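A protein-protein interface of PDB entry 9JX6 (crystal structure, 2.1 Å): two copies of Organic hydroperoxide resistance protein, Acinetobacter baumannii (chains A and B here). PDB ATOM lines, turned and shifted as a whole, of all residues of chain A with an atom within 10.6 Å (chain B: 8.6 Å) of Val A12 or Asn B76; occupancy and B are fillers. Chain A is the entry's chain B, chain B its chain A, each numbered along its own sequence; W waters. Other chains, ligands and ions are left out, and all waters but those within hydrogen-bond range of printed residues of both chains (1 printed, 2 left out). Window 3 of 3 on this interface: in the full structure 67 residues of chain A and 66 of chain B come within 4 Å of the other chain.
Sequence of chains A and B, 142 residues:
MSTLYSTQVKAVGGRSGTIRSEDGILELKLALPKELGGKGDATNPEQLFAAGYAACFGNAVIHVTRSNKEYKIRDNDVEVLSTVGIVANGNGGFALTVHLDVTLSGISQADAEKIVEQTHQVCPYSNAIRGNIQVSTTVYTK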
ATOM      1  N   VAL A   9      -9.667  -7.556 -25.545  1.00  0.00           N
ATOM      2  CA  VAL A   9     -10.924  -8.190 -25.165  1.00  0.00           C
ATOM      3  C   VAL A   9     -12.049  -7.601 -26.006  1.00  0.00           C
ATOM      4  O   VAL A   9     -12.125  -6.381 -26.196  1.00  0.00           O
ATOM      5  CB  VAL A   9     -11.225  -8.024 -23.662  1.00  0.00           C
ATOM      6  CG1 VAL A   9     -12.571  -8.663 -23.326  1.00  0.00           C
ATOM      7  CG2 VAL A   9     -10.125  -8.656 -22.832  1.00  0.00           C
ATOM      8  N   LYS A  10     -12.923  -8.472 -26.505  1.00  0.00           N
ATOM      9  CA  LYS A  10     -14.031  -8.092 -27.372  1.00  0.00           C
ATOM     10  C   LYS A  10     -15.329  -8.219 -26.589  1.00  0.00           C
ATOM     11  O   LYS A  10     -15.652  -9.302 -26.092  1.00  0.00           O
ATOM     12  CB  LYS A  10     -14.079  -8.978 -28.619  1.00  0.00           C
ATOM     13  CG  LYS A  10     -15.094  -8.544 -29.656  1.00  0.00           C
ATOM     14  CD  LYS A  10     -14.490  -8.532 -31.047  1.00  0.00           C
ATOM     15  CE  LYS A  10     -13.793  -9.834 -31.376  1.00  0.00           C
ATOM     16  NZ  LYS A  10     -14.673 -10.740 -32.164  1.00  0.00           N
ATOM     17  N   ALA A  11     -16.075  -7.123 -26.492  1.00  0.00           N
ATOM     18  CA  ALA A  11     -17.369  -7.114 -25.825  1.00  0.00           C
ATOM     19  C   ALA A  11     -18.462  -6.832 -26.844  1.00  0.00           C
ATOM     20  O   ALA A  11     -18.388  -5.843 -27.584  1.00  0.00           O
ATOM     21  CB  ALA A  11     -17.409  -6.074 -24.704  1.00  0.00           C
ATOM     22  N   VAL A  12     -19.475  -7.694 -26.873  1.00  0.00           N
ATOM     23  CA  VAL A  12     -20.598  -7.576 -27.796  1.00  0.00           C
ATOM     24  C   VAL A  12     -21.888  -7.567 -26.989  1.00  0.00           C
ATOM     25  O   VAL A  12     -22.130  -8.476 -26.187  1.00  0.00           O
ATOM     26  CB  VAL A  12     -20.616  -8.723 -28.823  1.00  0.00           C
ATOM     27  CG1 VAL A  12     -21.765  -8.533 -29.812  1.00  0.00           C
ATOM     28  CG2 VAL A  12     -19.283  -8.817 -29.549  1.00  0.00           C
ATOM     29  N   GLY A  13     -22.713  -6.547 -27.203  1.00  0.00           N
ATOM     30  CA  GLY A  13     -24.038  -6.512 -26.617  1.00  0.00           C
ATOM     31  C   GLY A  13     -24.165  -5.786 -25.298  1.00  0.00           C
ATOM     32  O   GLY A  13     -25.219  -5.884 -24.659  1.00  0.00           O
ATOM     33  N   GLY A  14     -23.133  -5.067 -24.863  1.00  0.00           N
ATOM     34  CA  GLY A  14     -23.259  -4.288 -23.647  1.00  0.00           C
ATOM     35  C   GLY A  14     -23.306  -5.147 -22.393  1.00  0.00           C
ATOM     36  O   GLY A  14     -22.687  -6.212 -22.303  1.00  0.00           O
ATOM     37  N   ARG A  15     -24.064  -4.669 -21.404  1.00  0.00           N
ATOM     38  CA  ARG A  15     -24.115  -5.310 -20.097  1.00  0.00           C
ATOM     39  C   ARG A  15     -24.954  -6.582 -20.082  1.00  0.00           C
ATOM     40  O   ARG A  15     -24.985  -7.269 -19.056  1.00  0.00           O
ATOM     41  CB  ARG A  15     -24.655  -4.328 -19.053  1.00  0.00           C
ATOM     42  CG  ARG A  15     -23.613  -3.348 -18.525  1.00  0.00           C
ATOM     43  CD  ARG A  15     -24.276  -2.157 -17.851  1.00  0.00           C
ATOM     44  NE  ARG A  15     -23.310  -1.156 -17.415  1.00  0.00           N
ATOM     45  CZ  ARG A  15     -22.656  -1.200 -16.262  1.00  0.00           C
ATOM     46  NH1 ARG A  15     -22.835  -2.191 -15.404  1.00  0.00           N
ATOM     47  NH2 ARG A  15     -21.805  -0.224 -15.960  1.00  0.00           N
ATOM     48  N   SER A  16     -25.633  -6.911 -21.179  1.00  0.00           N
ATOM     49  CA  SER A  16     -26.382  -8.156 -21.289  1.00  0.00           C
ATOM     50  C   SER A  16     -25.765  -9.113 -22.299  1.00  0.00           C
ATOM     51  O   SER A  16     -26.377 -10.138 -22.620  1.00  0.00           O
ATOM     52  CB  SER A  16     -27.839  -7.869 -21.657  1.00  0.00           C
ATOM     53  OG  SER A  16     -28.508  -7.184 -20.610  1.00  0.00           O
ATOM     54  N   GLY A  17     -24.578  -8.809 -22.801  1.00  0.00           N
ATOM     55  CA  GLY A  17     -23.948  -9.577 -23.858  1.00  0.00           C
ATOM     56  C   GLY A  17     -22.821 -10.455 -23.364  1.00  0.00           C
ATOM     57  O   GLY A  17     -22.929 -11.105 -22.322  1.00  0.00           O
ATOM     58  N   THR A  18     -21.726 -10.474 -24.124  1.00  0.00           N
ATOM     59  CA  THR A  18     -20.617 -11.383 -23.881  1.00  0.00           C
ATOM     60  C   THR A  18     -19.299 -10.626 -23.934  1.00  0.00           C
ATOM     61  O   THR A  18     -19.212  -9.514 -24.463  1.00  0.00           O
ATOM     62  CB  THR A  18     -20.584 -12.520 -24.912  1.00  0.00           C
ATOM     63  OG1 THR A  18     -20.353 -11.971 -26.216  1.00  0.00           O
ATOM     64  CG2 THR A  18     -21.901 -13.291 -24.916  1.00  0.00           C
ATOM     65  N   ILE A  19     -18.264 -11.252 -23.379  1.00  0.00           N
ATOM     66  CA  ILE A  19     -16.893 -10.762 -23.475  1.00  0.00           C
ATOM     67  C   ILE A  19     -15.988 -11.948 -23.770  1.00  0.00           C
ATOM     68  O   ILE A  19     -16.225 -13.058 -23.282  1.00  0.00           O
ATOM     69  CB  ILE A  19     -16.445 -10.038 -22.189  1.00  0.00           C
ATOM     70  CG1 ILE A  19     -16.720 -10.911 -20.967  1.00  0.00           C
ATOM     71  CG2 ILE A  19     -17.136  -8.692 -22.056  1.00  0.00           C
ATOM     72  CD1 ILE A  19     -15.619 -10.893 -19.950  1.00  0.00           C
ATOM     73  N   ARG A  20     -14.947 -11.714 -24.564  1.00  0.00           N
ATOM     74  CA  ARG A  20     -14.006 -12.773 -24.910  1.00  0.00           C
ATOM     75  C   ARG A  20     -12.674 -12.146 -25.278  1.00  0.00           C
ATOM     76  O   ARG A  20     -12.609 -11.324 -26.197  1.00  0.00           O
ATOM     77  CB  ARG A  20     -14.536 -13.626 -26.063  1.00  0.00           C
ATOM     78  CG  ARG A  20     -13.602 -14.748 -26.475  1.00  0.00           C
ATOM     79  CD  ARG A  20     -14.067 -15.424 -27.757  1.00  0.00           C
ATOM     80  NE  ARG A  20     -13.204 -16.542 -28.121  1.00  0.00           N
ATOM     81  CZ  ARG A  20     -12.037 -16.419 -28.736  1.00  0.00           C
ATOM     82  NH1 ARG A  20     -11.565 -15.236 -29.093  1.00  0.00           N
ATOM     83  NH2 ARG A  20     -11.325 -17.510 -29.003  1.00  0.00           N
ATOM     84  N   SER A  21     -11.623 -12.526 -24.559  1.00  0.00           N
ATOM     85  CA  SER A  21     -10.284 -12.109 -24.939  1.00  0.00           C
ATOM     86  C   SER A  21      -9.893 -12.769 -26.255  1.00  0.00           C
ATOM     87  O   SER A  21     -10.389 -13.843 -26.609  1.00  0.00           O
ATOM     88  CB  SER A  21      -9.276 -12.469 -23.848  1.00  0.00           C
ATOM     89  OG  SER A  21      -9.277 -13.862 -23.582  1.00  0.00           O
ATOM     90  N   GLU A  22      -8.996 -12.111 -26.990  1.00  0.00           N
ATOM     91  CA  GLU A  22      -8.603 -12.633 -28.291  1.00  0.00           C
ATOM     92  C   GLU A  22      -7.798 -13.920 -28.175  1.00  0.00           C
ATOM     93  O   GLU A  22      -7.759 -14.696 -29.136  1.00  0.00           O
ATOM     94  CB  GLU A  22      -7.812 -11.581 -29.066  1.00  0.00           C
ATOM     95  CG  GLU A  22      -8.674 -10.442 -29.589  1.00  0.00           C
ATOM     96  CD  GLU A  22      -9.627 -10.888 -30.680  1.00  0.00           C
ATOM     97  OE1 GLU A  22      -9.172 -11.540 -31.644  1.00  0.00           O
ATOM     98  OE2 GLU A  22     -10.835 -10.591 -30.570  1.00  0.00           O
ATOM     99  N   GLU A  27     -13.420 -15.704 -21.273  1.00  0.00           N
ATOM    100  CA  GLU A  27     -14.631 -15.755 -22.088  1.00  0.00           C
ATOM    101  C   GLU A  27     -15.799 -16.086 -21.175  1.00  0.00           C
ATOM    102  O   GLU A  27     -15.801 -17.147 -20.542  1.00  0.00           O
ATOM    103  CB  GLU A  27     -14.497 -16.798 -23.201  1.00  0.00           C
ATOM    104  CG  GLU A  27     -15.821 -17.373 -23.684  1.00  0.00           C
ATOM    105  CD  GLU A  27     -15.819 -17.675 -25.168  1.00  0.00           C
ATOM    106  OE1 GLU A  27     -14.869 -18.337 -25.638  1.00  0.00           O
ATOM    107  OE2 GLU A  27     -16.769 -17.257 -25.863  1.00  0.00           O
ATOM    108  N   LEU A  28     -16.775 -15.185 -21.093  1.00  0.00           N
ATOM    109  CA  LEU A  28     -17.936 -15.422 -20.248  1.00  0.00           C
ATOM    110  C   LEU A  28     -19.044 -14.448 -20.619  1.00  0.00           C
ATOM    111  O   LEU A  28     -18.810 -13.418 -21.258  1.00  0.00           O
ATOM    112  CB  LEU A  28     -17.592 -15.315 -18.754  1.00  0.00           C
ATOM    113  CG  LEU A  28     -16.897 -14.091 -18.154  1.00  0.00           C
ATOM    114  CD1 LEU A  28     -17.141 -14.073 -16.663  1.00  0.00           C
ATOM    115  CD2 LEU A  28     -15.409 -14.132 -18.403  1.00  0.00           C
ATOM    116  N   LYS A  29     -20.260 -14.802 -20.218  1.00  0.00           N
ATOM    117  CA  LYS A  29     -21.445 -14.002 -20.474  1.00  0.00           C
ATOM    118  C   LYS A  29     -21.637 -12.988 -19.352  1.00  0.00           C
ATOM    119  O   LYS A  29     -21.139 -13.158 -18.237  1.00  0.00           O
ATOM    120  CB  LYS A  29     -22.673 -14.912 -20.620  1.00  0.00           C
ATOM    121  CG  LYS A  29     -24.024 -14.205 -20.680  1.00  0.00           C
ATOM    122  CD  LYS A  29     -24.804 -14.592 -21.927  1.00  0.00           C
ATOM    123  CE  LYS A  29     -25.892 -13.573 -22.236  1.00  0.00           C
ATOM    124  NZ  LYS A  29     -25.620 -12.821 -23.493  1.00  0.00           N
ATOM    125  N   LEU A  30     -22.342 -11.904 -19.669  1.00  0.00           N
ATOM    126  CA  LEU A  30     -22.673 -10.868 -18.706  1.00  0.00           C
ATOM    127  C   LEU A  30     -24.181 -10.791 -18.521  1.00  0.00           C
ATOM    128  O   LEU A  30     -24.954 -11.120 -19.424  1.00  0.00           O
ATOM    129  CB  LEU A  30     -22.159  -9.497 -19.143  1.00  0.00           C
ATOM    130  CG  LEU A  30     -20.705  -9.336 -19.577  1.00  0.00           C
ATOM    131  CD1 LEU A  30     -20.370  -7.872 -19.554  1.00  0.00           C
ATOM    132  CD2 LEU A  30     -19.759 -10.105 -18.680  1.00  0.00           C
ATOM    133  N   ALA A  31     -24.589 -10.333 -17.342  1.00  0.00           N
ATOM    134  CA  ALA A  31     -25.991 -10.099 -17.048  1.00  0.00           C
ATOM    135  C   ALA A  31     -26.113  -8.868 -16.166  1.00  0.00           C
ATOM    136  O   ALA A  31     -25.233  -8.576 -15.352  1.00  0.00           O
ATOM    137  CB  ALA A  31     -26.638 -11.309 -16.359  1.00  0.00           C
ATOM    138  N   PRO A  45     -19.612  -5.510 -15.503  1.00  0.00           N
ATOM    139  CA  PRO A  45     -18.394  -4.684 -15.528  1.00  0.00           C
ATOM    140  C   PRO A  45     -17.864  -4.319 -14.151  1.00  0.00           C
ATOM    141  O   PRO A  45     -16.642  -4.311 -13.950  1.00  0.00           O
ATOM    142  CB  PRO A  45     -18.843  -3.443 -16.310  1.00  0.00           C
ATOM    143  CG  PRO A  45     -19.882  -3.970 -17.238  1.00  0.00           C
ATOM    144  CD  PRO A  45     -20.645  -4.975 -16.416  1.00  0.00           C
ATOM    145  N   LEU A  48     -16.011  -7.235 -12.754  1.00  0.00           N
ATOM    146  CA  LEU A  48     -14.745  -7.441 -13.452  1.00  0.00           C
ATOM    147  C   LEU A  48     -13.707  -6.406 -13.030  1.00  0.00           C
ATOM    148  O   LEU A  48     -12.540  -6.745 -12.799  1.00  0.00           O
ATOM    149  CB  LEU A  48     -14.974  -7.393 -14.965  1.00  0.00           C
ATOM    150  CG  LEU A  48     -15.754  -8.566 -15.569  1.00  0.00           C
ATOM    151  CD1 LEU A  48     -16.289  -8.211 -16.952  1.00  0.00           C
ATOM    152  CD2 LEU A  48     -14.894  -9.821 -15.629  1.00  0.00           C
ATOM    153  N   ALA B  51     -12.073  -6.163 -20.255  1.00  0.00           N
ATOM    154  CA  ALA B  51     -13.404  -6.741 -20.405  1.00  0.00           C
ATOM    155  C   ALA B  51     -14.467  -5.849 -19.776  1.00  0.00           C
ATOM    156  O   ALA B  51     -15.520  -5.602 -20.377  1.00  0.00           O
ATOM    157  CB  ALA B  51     -13.438  -8.138 -19.786  1.00  0.00           C
ATOM    158  N   ALA B  54     -14.722  -2.487 -21.938  1.00  0.00           N
ATOM    159  CA  ALA B  54     -15.378  -2.706 -23.223  1.00  0.00           C
ATOM    160  C   ALA B  54     -16.865  -2.990 -23.053  1.00  0.00           C
ATOM    161  O   ALA B  54     -17.670  -2.614 -23.911  1.00  0.00           O
ATOM    162  CB  ALA B  54     -14.700  -3.853 -23.970  1.00  0.00           C
ATOM    163  N   ALA B  55     -17.248  -3.631 -21.948  1.00  0.00           N
ATOM    164  CA  ALA B  55     -18.653  -3.945 -21.719  1.00  0.00           C
ATOM    165  C   ALA B  55     -19.453  -2.718 -21.290  1.00  0.00           C
ATOM    166  O   ALA B  55     -20.590  -2.537 -21.738  1.00  0.00           O
ATOM    167  CB  ALA B  55     -18.772  -5.055 -20.681  1.00  0.00           C
ATOM    168  N   GLY B  58     -19.722  -0.292 -24.517  1.00  0.00           N
ATOM    169  CA  GLY B  58     -20.712  -0.815 -25.441  1.00  0.00           C
ATOM    170  C   GLY B  58     -22.131  -0.629 -24.938  1.00  0.00           C
ATOM    171  O   GLY B  58     -23.017  -0.219 -25.691  1.00  0.00           O
ATOM    172  N   ASN B  59     -22.362  -0.915 -23.654  1.00  0.00           N
ATOM    173  CA  ASN B  59     -23.689  -0.707 -23.086  1.00  0.00           C
ATOM    174  C   ASN B  59     -24.062   0.770 -23.074  1.00  0.00           C
ATOM    175  O   ASN B  59     -25.208   1.129 -23.370  1.00  0.00           O
ATOM    176  CB  ASN B  59     -23.759  -1.284 -21.674  1.00  0.00           C
ATOM    177  CG  ASN B  59     -25.184  -1.474 -21.199  1.00  0.00           C
ATOM    178  OD1 ASN B  59     -25.815  -2.493 -21.483  1.00  0.00           O
ATOM    179  ND2 ASN B  59     -25.705  -0.483 -20.490  1.00  0.00           N
ATOM    180  N   ILE B  62     -25.104   1.873 -26.528  1.00  0.00           N
ATOM    181  CA  ILE B  62     -26.489   1.514 -26.822  1.00  0.00           C
ATOM    182  C   ILE B  62     -27.442   2.543 -26.231  1.00  0.00           C
ATOM    183  O   ILE B  62     -28.404   2.969 -26.882  1.00  0.00           O
ATOM    184  CB  ILE B  62     -26.793   0.098 -26.300  1.00  0.00           C
ATOM    185  CG1 ILE B  62     -25.954  -0.941 -27.043  1.00  0.00           C
ATOM    186  CG2 ILE B  62     -28.273  -0.218 -26.432  1.00  0.00           C
ATOM    187  CD1 ILE B  62     -25.889  -2.285 -26.345  1.00  0.00           C
ATOM    188  N   ARG B  66     -29.893   5.132 -28.362  1.00  0.00           N
ATOM    189  CA  ARG B  66     -31.330   5.083 -28.125  1.00  0.00           C
ATOM    190  C   ARG B  66     -31.854   6.317 -27.401  1.00  0.00           C
ATOM    191  O   ARG B  66     -33.060   6.403 -27.153  1.00  0.00           O
ATOM    192  CB  ARG B  66     -31.689   3.823 -27.334  1.00  0.00           C
ATOM    193  CG  ARG B  66     -31.528   2.535 -28.131  1.00  0.00           C
ATOM    194  CD  ARG B  66     -31.803   1.309 -27.275  1.00  0.00           C
ATOM    195  NE  ARG B  66     -31.498   0.073 -27.985  1.00  0.00           N
ATOM    196  CZ  ARG B  66     -31.419  -1.120 -27.412  1.00  0.00           C
ATOM    197  NH1 ARG B  66     -31.626  -1.278 -26.115  1.00  0.00           N
ATOM    198  NH2 ARG B  66     -31.119  -2.180 -28.157  1.00  0.00           N
ATOM    199  N   ILE B  73     -31.733   0.391 -32.826  1.00  0.00           N
ATOM    200  CA  ILE B  73     -30.546  -0.454 -32.778  1.00  0.00           C
ATOM    201  C   ILE B  73     -30.718  -1.493 -31.680  1.00  0.00           C
ATOM    202  O   ILE B  73     -31.190  -1.181 -30.582  1.00  0.00           O
ATOM    203  CB  ILE B  73     -29.281   0.398 -32.546  1.00  0.00           C
ATOM    204  CG1 ILE B  73     -28.088  -0.475 -32.166  1.00  0.00           C
ATOM    205  CG2 ILE B  73     -29.535   1.433 -31.465  1.00  0.00           C
ATOM    206  CD1 ILE B  73     -26.820   0.313 -31.959  1.00  0.00           C
ATOM    207  N   ARG B  74     -30.344  -2.733 -31.979  1.00  0.00           N
ATOM    208  CA  ARG B  74     -30.374  -3.808 -31.001  1.00  0.00           C
ATOM    209  C   ARG B  74     -28.995  -4.011 -30.382  1.00  0.00           C
ATOM    210  O   ARG B  74     -27.981  -3.528 -30.890  1.00  0.00           O
ATOM    211  CB  ARG B  74     -30.884  -5.110 -31.629  1.00  0.00           C
ATOM    212  CG  ARG B  74     -30.194  -5.524 -32.912  1.00  0.00           C
ATOM    213  CD  ARG B  74     -31.210  -5.629 -34.040  1.00  0.00           C
ATOM    214  NE  ARG B  74     -30.686  -6.358 -35.188  1.00  0.00           N
ATOM    215  CZ  ARG B  74     -31.303  -6.460 -36.357  1.00  0.00           C
ATOM    216  NH1 ARG B  74     -32.465  -5.866 -36.579  1.00  0.00           N
ATOM    217  NH2 ARG B  74     -30.745  -7.181 -37.325  1.00  0.00           N
ATOM    218  N   ASP B  75     -28.984  -4.743 -29.264  1.00  0.00           N
ATOM    219  CA  ASP B  75     -27.800  -4.839 -28.411  1.00  0.00           C
ATOM    220  C   ASP B  75     -26.562  -5.276 -29.186  1.00  0.00           C
ATOM    221  O   ASP B  75     -25.492  -4.670 -29.064  1.00  0.00           O
ATOM    222  CB  ASP B  75     -28.069  -5.811 -27.262  1.00  0.00           C
ATOM    223  CG  ASP B  75     -28.832  -5.170 -26.121  1.00  0.00           C
ATOM    224  OD1 ASP B  75     -29.407  -4.081 -26.325  1.00  0.00           O
ATOM    225  OD2 ASP B  75     -28.856  -5.756 -25.018  1.00  0.00           O
ATOM    226  N   ASN B  76     -26.687  -6.331 -29.985  1.00  0.00           N
ATOM    227  CA  ASN B  76     -25.531  -6.900 -30.664  1.00  0.00           C
ATOM    228  C   ASN B  76     -25.112  -6.113 -31.901  1.00  0.00           C
ATOM    229  O   ASN B  76     -24.226  -6.567 -32.632  1.00  0.00           O
ATOM    230  CB  ASN B  76     -25.805  -8.360 -31.031  1.00  0.00           C
ATOM    231  CG  ASN B  76     -25.756  -9.277 -29.824  1.00  0.00           C
ATOM    232  OD1 ASN B  76     -25.573  -8.824 -28.693  1.00  0.00           O
ATOM    233  ND2 ASN B  76     -25.919 -10.574 -30.058  1.00  0.00           N
ATOM    234  N   ASP B  77     -25.717  -4.956 -32.155  1.00  0.00           N
ATOM    235  CA  ASP B  77     -25.210  -4.049 -33.175  1.00  0.00           C
ATOM    236  C   ASP B  77     -24.057  -3.193 -32.669  1.00  0.00           C
ATOM    237  O   ASP B  77     -23.579  -2.323 -33.406  1.00  0.00           O
ATOM    238  CB  ASP B  77     -26.330  -3.144 -33.695  1.00  0.00           C
ATOM    239  CG  ASP B  77     -27.317  -3.880 -34.581  1.00  0.00           C
ATOM    240  OD1 ASP B  77     -26.950  -4.932 -35.146  1.00  0.00           O
ATOM    241  OD2 ASP B  77     -28.461  -3.397 -34.723  1.00  0.00           O
ATOM    242  N   VAL B  78     -23.608  -3.413 -31.434  1.00  0.00           N
ATOM    243  CA  VAL B  78     -22.512  -2.658 -30.840  1.00  0.00           C
ATOM    244  C   VAL B  78     -21.435  -3.636 -30.401  1.00  0.00           C
ATOM    245  O   VAL B  78     -21.719  -4.613 -29.700  1.00  0.00           O
ATOM    246  CB  VAL B  78     -22.975  -1.798 -29.649  1.00  0.00           C
ATOM    247  CG1 VAL B  78     -21.785  -1.076 -29.028  1.00  0.00           C
ATOM    248  CG2 VAL B  78     -24.015  -0.797 -30.101  1.00  0.00           C
ATOM    249  N   GLU B  79     -20.202  -3.366 -30.811  1.00  0.00           N
ATOM    250  CA  GLU B  79     -19.046  -4.179 -30.473  1.00  0.00           C
ATOM    251  C   GLU B  79     -17.904  -3.262 -30.075  1.00  0.00           C
ATOM    252  O   GLU B  79     -17.614  -2.291 -30.778  1.00  0.00           O
ATOM    253  CB  GLU B  79     -18.641  -5.066 -31.652  1.00  0.00           C
ATOM    254  CG  GLU B  79     -17.516  -6.024 -31.351  1.00  0.00           C
ATOM    255  CD  GLU B  79     -16.816  -6.462 -32.617  1.00  0.00           C
ATOM    256  OE1 GLU B  79     -17.447  -7.144 -33.447  1.00  0.00           O
ATOM    257  OE2 GLU B  79     -15.651  -6.064 -32.818  1.00  0.00           O
ATOM    258  N   VAL B  80     -17.268  -3.563 -28.947  1.00  0.00           N
ATOM    259  CA  VAL B  80     -16.130  -2.795 -28.460  1.00  0.00           C
ATOM    260  C   VAL B  80     -14.958  -3.749 -28.286  1.00  0.00           C
ATOM    261  O   VAL B  80     -15.063  -4.752 -27.569  1.00  0.00           O
ATOM    262  CB  VAL B  80     -16.447  -2.064 -27.147  1.00  0.00           C
ATOM    263  CG1 VAL B  80     -15.204  -1.359 -26.625  1.00  0.00           C
ATOM    264  CG2 VAL B  80     -17.583  -1.069 -27.358  1.00  0.00           C
ATOM    265  N   LEU B  81     -13.850  -3.443 -28.948  1.00  0.00           N
ATOM    266  CA  LEU B  81     -12.612  -4.199 -28.816  1.00  0.00           C
ATOM    267  C   LEU B  81     -11.617  -3.312 -28.085  1.00  0.00           C
ATOM    268  O   LEU B  81     -11.096  -2.349 -28.659  1.00  0.00           O
ATOM    269  CB  LEU B  81     -12.074  -4.627 -30.180  1.00  0.00           C
ATOM    270  CG  LEU B  81     -10.762  -5.412 -30.139  1.00  0.00           C
ATOM    271  CD1 LEU B  81     -11.001  -6.842 -29.667  1.00  0.00           C
ATOM    272  CD2 LEU B  81     -10.079  -5.392 -31.498  1.00  0.00           C
ATOM    273  N   THR B 103     -17.324  -0.557 -32.924  1.00  0.00           N
ATOM    274  CA  THR B 103     -17.986  -0.862 -34.187  1.00  0.00           C
ATOM    275  C   THR B 103     -19.495  -0.838 -33.981  1.00  0.00           C
ATOM    276  O   THR B 103     -20.029  -1.610 -33.177  1.00  0.00           O
ATOM    277  CB  THR B 103     -17.530  -2.223 -34.726  1.00  0.00           C
ATOM    278  OG1 THR B 103     -16.101  -2.236 -34.862  1.00  0.00           O
ATOM    279  CG2 THR B 103     -18.164  -2.502 -36.074  1.00  0.00           C
ATOM    280  N   LEU B 104     -20.178   0.042 -34.713  1.00  0.00           N
ATOM    281  CA  LEU B 104     -21.627   0.215 -34.629  1.00  0.00           C
ATOM    282  C   LEU B 104     -22.262  -0.199 -35.950  1.00  0.00           C
ATOM    283  O   LEU B 104     -21.912   0.343 -37.000  1.00  0.00           O
ATOM    284  CB  LEU B 104     -21.993   1.666 -34.311  1.00  0.00           C
ATOM    285  CG  LEU B 104     -21.913   2.238 -32.890  1.00  0.00           C
ATOM    286  CD1 LEU B 104     -20.588   1.953 -32.222  1.00  0.00           C
ATOM    287  CD2 LEU B 104     -22.221   3.747 -32.900  1.00  0.00           C
ATOM    288  N   SER B 105     -23.209  -1.132 -35.894  1.00  0.00           N
ATOM    289  CA  SER B 105     -23.854  -1.641 -37.097  1.00  0.00           C
ATOM    290  C   SER B 105     -25.033  -0.763 -37.503  1.00  0.00           C
ATOM    291  O   SER B 105     -25.827  -0.333 -36.662  1.00  0.00           O
ATOM    292  CB  SER B 105     -24.325  -3.080 -36.881  1.00  0.00           C
ATOM    293  OG  SER B 105     -23.218  -3.940 -36.680  1.00  0.00           O
ATOM    294  N   LYS B 142     -19.192  -0.880 -39.886  1.00  0.00           N
ATOM    295  CA  LYS B 142     -19.620  -2.216 -40.316  1.00  0.00           C
ATOM    296  C   LYS B 142     -20.785  -2.196 -41.311  1.00  0.00           C
ATOM    297  O   LYS B 142     -21.949  -2.357 -40.932  1.00  0.00           O
ATOM    298  CB  LYS B 142     -20.002  -3.063 -39.099  1.00  0.00           C
ATOM    299  CG  LYS B 142     -20.184  -4.540 -39.401  1.00  0.00           C
ATOM    300  CD  LYS B 142     -19.239  -5.392 -38.567  1.00  0.00           C
ATOM    301  CE  LYS B 142     -19.985  -6.148 -37.479  1.00  0.00           C
ATOM    302  NZ  LYS B 142     -19.084  -7.078 -36.742  1.00  0.00           N
HETATM  303  O   HOH W   1     -20.311  -4.200 -25.430  1.00  0.00           O
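Val A12 touches just these residues of chain B: Asn B76, Val B78 and Glu B79. Asn B76 touches two residues of chain A. Of chain A, only Gly A13 comes within 4 Å of Asp B75. Asp B77 touches none of the printed residues of chain A. Printed residues of chain A within 4 Å of Val B80: Val A9 (3.6 Å), Lys A10 (3.5 Å) and Ala A11 (2.8 Å). Of the printed residues of chain B, Arg A15 touches Asn B59 (2.8 Å). Printed residues of chain A within 4 Å of Val B78: Val A12 and Gly A13. Of the printed residues of chain A, Leu B81 touches Val A9 (3.4 Å), Lys A10 (3.9 Å) and Glu A22 (3.9 Å). Printed residues of chain B within 4 Å of Lys A10: Glu B79, Val B80 and Leu B81. Leu B104 touches none of the printed residues of chain A. Lys B142 touches none of the printed residues of chain A. The nearest residue of chain A that does not touch Asn B76 is Gly A17 (5.2 Å).
Water W1 lies within hydrogen-bond range of the backbone NH of Gly A14 (3.0 Å), the backbone carbonyl oxygen of Ala A11 (3.3 Å) and the backbone carbonyl oxygen of Ala B54 (3.4 Å).
Among the printed residues, merely in contact across the chains: Val A9 with Ala B51, Val A9 with Val B80, Val A9 with Leu B81, Lys A10 with Glu B79, Lys A10 with Val B80, Lys A10 with Leu B81, Ala A11 with Ala B54, Ala A11 with Ala B55, Ala A11 with Glu B79, Val A12 with Asn B76, Val A12 with Val B78, Val A12 with Glu B79, Gly A13 with Asp B75, Gly A13 with Asn B76, Gly A14 with Ala B55, Gly A14 with Asn B59, Ile A19 with Ala B51, Glu A22 with Leu B81, Leu A30 with Ala B55 and Pro A45 with Ala B55.
No position is printed for both chains.
O of Val B80 sits at hydrogen-bond distance from N of Ala A11 (2.8 Å). N of Gly A13 is in hydrogen-bond range of O of Val B78, 3.3 Å away. N of Arg A15 is in hydrogen-bond range of OD1 of Asn B59 (2.8 Å).
Of the 21 printed residues of chain A, 11 touch a printed residue of chain B. Along chain A the printed residues that touch a printed residue of chain B span positions 9 to 45.
N of Lys A10 is in hydrogen-bond range of O of Arg A20 (2.9 Å). The backbone NH of Thr A18 is in hydrogen-bond range of the backbone carbonyl oxygen of Val A12 (2.9 Å). O of Gly A17 is in hydrogen-bond range of N of Leu A30, at 2.8 Å. The backbone NH (N) of Ile A19 is in hydrogen-bond range of the backbone carbonyl oxygen (O) of Leu A28. The guanidinium group (NH2) of Arg B66 lies within salt-bridge range of the side-chain carboxylate (OD1) of Asp B75 (3.1 Å). The backbone carbonyl oxygen of Glu B79 is in hydrogen-bond range of the backbone NH of Thr B103 (2.8 Å).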
